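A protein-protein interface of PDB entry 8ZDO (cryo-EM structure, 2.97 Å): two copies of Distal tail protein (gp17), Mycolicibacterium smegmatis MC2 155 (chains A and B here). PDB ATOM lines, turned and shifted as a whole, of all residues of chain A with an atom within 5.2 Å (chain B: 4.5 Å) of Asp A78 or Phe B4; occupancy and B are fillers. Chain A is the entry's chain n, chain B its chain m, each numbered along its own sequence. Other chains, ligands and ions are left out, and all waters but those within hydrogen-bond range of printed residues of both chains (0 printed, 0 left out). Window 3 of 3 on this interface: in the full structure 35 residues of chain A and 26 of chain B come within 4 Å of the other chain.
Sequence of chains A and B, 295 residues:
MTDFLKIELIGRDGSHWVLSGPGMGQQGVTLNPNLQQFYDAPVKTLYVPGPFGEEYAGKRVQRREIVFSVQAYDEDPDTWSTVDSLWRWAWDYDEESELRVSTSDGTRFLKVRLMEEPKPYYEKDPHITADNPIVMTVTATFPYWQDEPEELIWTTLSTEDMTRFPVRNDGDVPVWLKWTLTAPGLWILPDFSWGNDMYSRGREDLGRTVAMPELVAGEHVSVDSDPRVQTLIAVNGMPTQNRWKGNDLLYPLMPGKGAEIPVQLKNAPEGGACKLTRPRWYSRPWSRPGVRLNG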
ATOM      1  N   ASP A  76      -0.353  -1.330   7.160  1.00  0.00           N
ATOM      2  CA  ASP A  76      -1.288  -2.301   7.695  1.00  0.00           C
ATOM      3  C   ASP A  76      -0.602  -3.641   7.935  1.00  0.00           C
ATOM      4  O   ASP A  76       0.218  -4.077   7.118  1.00  0.00           O
ATOM      5  CB  ASP A  76      -2.484  -2.497   6.752  1.00  0.00           C
ATOM      6  CG  ASP A  76      -2.065  -2.711   5.317  1.00  0.00           C
ATOM      7  OD1 ASP A  76      -1.009  -2.176   4.921  1.00  0.00           O
ATOM      8  OD2 ASP A  76      -2.794  -3.412   4.583  1.00  0.00           O
ATOM      9  N   PRO A  77      -0.912  -4.307   9.051  1.00  0.00           N
ATOM     10  CA  PRO A  77      -0.233  -5.573   9.370  1.00  0.00           C
ATOM     11  C   PRO A  77      -0.433  -6.667   8.338  1.00  0.00           C
ATOM     12  O   PRO A  77       0.483  -7.468   8.127  1.00  0.00           O
ATOM     13  CB  PRO A  77      -0.843  -5.958  10.724  1.00  0.00           C
ATOM     14  CG  PRO A  77      -1.308  -4.670  11.304  1.00  0.00           C
ATOM     15  CD  PRO A  77      -1.783  -3.856  10.147  1.00  0.00           C
ATOM     16  N   ASP A  78      -1.592  -6.733   7.685  1.00  0.00           N
ATOM     17  CA  ASP A  78      -1.813  -7.774   6.685  1.00  0.00           C
ATOM     18  C   ASP A  78      -0.867  -7.608   5.502  1.00  0.00           C
ATOM     19  O   ASP A  78      -0.226  -8.570   5.055  1.00  0.00           O
ATOM     20  CB  ASP A  78      -3.267  -7.745   6.221  1.00  0.00           C
ATOM     21  CG  ASP A  78      -4.217  -8.308   7.258  1.00  0.00           C
ATOM     22  OD1 ASP A  78      -4.029  -9.474   7.667  1.00  0.00           O
ATOM     23  OD2 ASP A  78      -5.150  -7.585   7.666  1.00  0.00           O
ATOM     24  N   THR A  79      -0.751  -6.384   4.989  1.00  0.00           N
ATOM     25  CA  THR A  79       0.144  -6.169   3.863  1.00  0.00           C
ATOM     26  C   THR A  79       1.596  -6.262   4.300  1.00  0.00           C
ATOM     27  O   THR A  79       2.452  -6.695   3.518  1.00  0.00           O
ATOM     28  CB  THR A  79      -0.132  -4.820   3.209  1.00  0.00           C
ATOM     29  OG1 THR A  79      -1.528  -4.715   2.917  1.00  0.00           O
ATOM     30  CG2 THR A  79       0.601  -4.752   1.890  1.00  0.00           C
ATOM     31  N   TRP A  80       1.896  -5.888   5.547  1.00  0.00           N
ATOM     32  CA  TRP A  80       3.240  -6.125   6.058  1.00  0.00           C
ATOM     33  C   TRP A  80       3.561  -7.612   6.056  1.00  0.00           C
ATOM     34  O   TRP A  80       4.682  -8.010   5.732  1.00  0.00           O
ATOM     35  CB  TRP A  80       3.408  -5.565   7.472  1.00  0.00           C
ATOM     36  CG  TRP A  80       4.643  -6.130   8.108  1.00  0.00           C
ATOM     37  CD1 TRP A  80       5.908  -5.629   8.031  1.00  0.00           C
ATOM     38  CD2 TRP A  80       4.740  -7.340   8.868  1.00  0.00           C
ATOM     39  NE1 TRP A  80       6.781  -6.441   8.709  1.00  0.00           N
ATOM     40  CE2 TRP A  80       6.087  -7.500   9.229  1.00  0.00           C
ATOM     41  CE3 TRP A  80       3.814  -8.298   9.283  1.00  0.00           C
ATOM     42  CZ2 TRP A  80       6.527  -8.576   9.984  1.00  0.00           C
ATOM     43  CZ3 TRP A  80       4.254  -9.364  10.023  1.00  0.00           C
ATOM     44  CH2 TRP A  80       5.596  -9.500  10.363  1.00  0.00           C
ATOM     45  N   SER A  81       2.594  -8.443   6.446  1.00  0.00           N
ATOM     46  CA  SER A  81       2.813  -9.884   6.453  1.00  0.00           C
ATOM     47  C   SER A  81       3.032 -10.406   5.041  1.00  0.00           C
ATOM     48  O   SER A  81       3.883 -11.274   4.816  1.00  0.00           O
ATOM     49  CB  SER A  81       1.633 -10.588   7.117  1.00  0.00           C
ATOM     50  OG  SER A  81       1.946 -11.936   7.411  1.00  0.00           O
ATOM     51  N   THR A  82       2.278  -9.876   4.078  1.00  0.00           N
ATOM     52  CA  THR A  82       2.507 -10.246   2.684  1.00  0.00           C
ATOM     53  C   THR A  82       3.926  -9.892   2.249  1.00  0.00           C
ATOM     54  O   THR A  82       4.623 -10.707   1.632  1.00  0.00           O
ATOM     55  CB  THR A  82       1.483  -9.560   1.782  1.00  0.00           C
ATOM     56  OG1 THR A  82       0.180 -10.095   2.042  1.00  0.00           O
ATOM     57  CG2 THR A  82       1.827  -9.786   0.325  1.00  0.00           C
ATOM     58  N   HIS A 127       3.217  -7.966  14.264  1.00  0.00           N
ATOM     59  CA  HIS A 127       2.000  -7.350  13.750  1.00  0.00           C
ATOM     60  C   HIS A 127       1.648  -6.059  14.474  1.00  0.00           C
ATOM     61  O   HIS A 127       0.822  -5.291  13.971  1.00  0.00           O
ATOM     62  CB  HIS A 127       0.831  -8.327  13.845  1.00  0.00           C
ATOM     63  CG  HIS A 127       1.003  -9.557  13.011  1.00  0.00           C
ATOM     64  ND1 HIS A 127       1.656 -10.679  13.468  1.00  0.00           N
ATOM     65  CD2 HIS A 127       0.608  -9.840  11.748  1.00  0.00           C
ATOM     66  CE1 HIS A 127       1.658 -11.601  12.523  1.00  0.00           C
ATOM     67  NE2 HIS A 127       1.028 -11.117  11.469  1.00  0.00           N
ATOM     68  N   THR B   2      -2.223  -9.280  19.646  1.00  0.00           N
ATOM     69  CA  THR B   2      -3.029  -8.683  18.589  1.00  0.00           C
ATOM     70  C   THR B   2      -4.015  -9.687  18.013  1.00  0.00           C
ATOM     71  O   THR B   2      -3.905 -10.887  18.253  1.00  0.00           O
ATOM     72  CB  THR B   2      -2.152  -8.137  17.453  1.00  0.00           C
ATOM     73  OG1 THR B   2      -1.183  -9.123  17.076  1.00  0.00           O
ATOM     74  CG2 THR B   2      -1.437  -6.874  17.894  1.00  0.00           C
ATOM     75  N   ASP B   3      -4.983  -9.187  17.247  1.00  0.00           N
ATOM     76  CA  ASP B   3      -5.961 -10.044  16.591  1.00  0.00           C
ATOM     77  C   ASP B   3      -5.458 -10.618  15.275  1.00  0.00           C
ATOM     78  O   ASP B   3      -6.193 -11.367  14.623  1.00  0.00           O
ATOM     79  CB  ASP B   3      -7.267  -9.277  16.375  1.00  0.00           C
ATOM     80  CG  ASP B   3      -7.084  -8.037  15.523  1.00  0.00           C
ATOM     81  OD1 ASP B   3      -5.934  -7.725  15.155  1.00  0.00           O
ATOM     82  OD2 ASP B   3      -8.095  -7.368  15.221  1.00  0.00           O
ATOM     83  N   PHE B   4      -4.238 -10.281  14.864  1.00  0.00           N
ATOM     84  CA  PHE B   4      -3.629 -10.862  13.678  1.00  0.00           C
ATOM     85  C   PHE B   4      -2.860 -12.141  13.968  1.00  0.00           C
ATOM     86  O   PHE B   4      -2.421 -12.807  13.027  1.00  0.00           O
ATOM     87  CB  PHE B   4      -2.686  -9.854  13.017  1.00  0.00           C
ATOM     88  CG  PHE B   4      -3.329  -8.537  12.705  1.00  0.00           C
ATOM     89  CD1 PHE B   4      -3.982  -8.340  11.503  1.00  0.00           C
ATOM     90  CD2 PHE B   4      -3.270  -7.493  13.609  1.00  0.00           C
ATOM     91  CE1 PHE B   4      -4.574  -7.132  11.213  1.00  0.00           C
ATOM     92  CE2 PHE B   4      -3.860  -6.281  13.324  1.00  0.00           C
ATOM     93  CZ  PHE B   4      -4.512  -6.101  12.125  1.00  0.00           C
ATOM     94  N   LEU B   5      -2.692 -12.501  15.238  1.00  0.00           N
ATOM     95  CA  LEU B   5      -1.868 -13.643  15.609  1.00  0.00           C
ATOM     96  C   LEU B   5      -2.373 -14.212  16.924  1.00  0.00           C
ATOM     97  O   LEU B   5      -2.637 -13.458  17.864  1.00  0.00           O
ATOM     98  CB  LEU B   5      -0.398 -13.232  15.733  1.00  0.00           C
ATOM     99  CG  LEU B   5       0.587 -14.207  16.374  1.00  0.00           C
ATOM    100  CD1 LEU B   5       0.708 -15.458  15.549  1.00  0.00           C
ATOM    101  CD2 LEU B   5       1.941 -13.549  16.532  1.00  0.00           C
ATOM    102  N   SER B 102      -1.982 -19.419  15.021  1.00  0.00           N
ATOM    103  CA  SER B 102      -3.106 -19.175  14.130  1.00  0.00           C
ATOM    104  C   SER B 102      -3.018 -17.754  13.597  1.00  0.00           C
ATOM    105  O   SER B 102      -2.953 -16.796  14.377  1.00  0.00           O
ATOM    106  CB  SER B 102      -4.436 -19.394  14.852  1.00  0.00           C
ATOM    107  OG  SER B 102      -5.525 -19.169  13.979  1.00  0.00           O
ATOM    108  N   THR B 103      -3.014 -17.626  12.274  1.00  0.00           N
ATOM    109  CA  THR B 103      -3.011 -16.342  11.585  1.00  0.00           C
ATOM    110  C   THR B 103      -3.959 -16.445  10.395  1.00  0.00           C
ATOM    111  O   THR B 103      -4.664 -17.444  10.222  1.00  0.00           O
ATOM    112  CB  THR B 103      -1.596 -15.953  11.139  1.00  0.00           C
ATOM    113  OG1 THR B 103      -0.973 -17.072  10.498  1.00  0.00           O
ATOM    114  CG2 THR B 103      -0.755 -15.515  12.315  1.00  0.00           C
ATOM    115  N   ARG B 288       2.724 -16.643   3.269  1.00  0.00           N
ATOM    116  CA  ARG B 288       1.814 -16.648   2.140  1.00  0.00           C
ATOM    117  C   ARG B 288       2.105 -17.848   1.242  1.00  0.00           C
ATOM    118  O   ARG B 288       3.255 -18.283   1.131  1.00  0.00           O
ATOM    119  CB  ARG B 288       1.943 -15.351   1.350  1.00  0.00           C
ATOM    120  CG  ARG B 288       1.540 -14.120   2.135  1.00  0.00           C
ATOM    121  CD  ARG B 288       0.044 -14.093   2.367  1.00  0.00           C
ATOM    122  NE  ARG B 288      -0.383 -12.885   3.060  1.00  0.00           N
ATOM    123  CZ  ARG B 288      -0.826 -12.856   4.309  1.00  0.00           C
ATOM    124  NH1 ARG B 288      -0.902 -13.954   5.040  1.00  0.00           N
ATOM    125  NH2 ARG B 288      -1.201 -11.696   4.837  1.00  0.00           N
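O of Asp A78 is in hydrogen-bond range of NH2 of Arg B288 (3.3 Å).
The guanidinium group (NE) of Arg B288 is in hydrogen-bond range of the side-chain hydroxyl (OG1) of Thr A82, at 3.0 Å.
O of Asp A78 lies within hydrogen-bond range of OG1 of Thr A82 (3.4 Å).
CG of Pro A77 touches CZ of Phe B4 (3.6 Å).
Phe B4 touches Asp A78 (CE1 to OD2, 3.6 Å).
Ser A81 touches Arg B288.
Thr B2 touches His A127 (OG1 to CB, 3.9 Å).
His A127 touches Phe B4 (CD2 to CB, 3.5 Å).
Leu B5 touches His A127.
Asp A78 touches two residues of chain B.
Of the printed residues of chain A, Leu B5 touches His A127 (3.98 Å).
Of the printed residues of chain A, Arg B288 touches Asp A78 (3.3 Å), Ser A81 (3.8 Å) and Thr A82 (3.0 Å).
Of the printed residues of chain A, Thr B2 touches His A127 (3.9 Å).
Of the printed residues of chain B, His A127 touches Thr B2 (3.9 Å), Phe B4 (3.5 Å) and Leu B5 (3.98 Å).
The nearest printed residue of chain B that does not touch Asp A78 is Thr B103 (7.5 Å).
Hydrophobic or aromatic side chains of chain B within 4 Å of the printed part of chain A: Phe B4 and Leu B5.
Hydrophobic or aromatic side chains of chain A that line the printed part of chain B: Pro A77 and His A127.
No position is printed for both chains.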
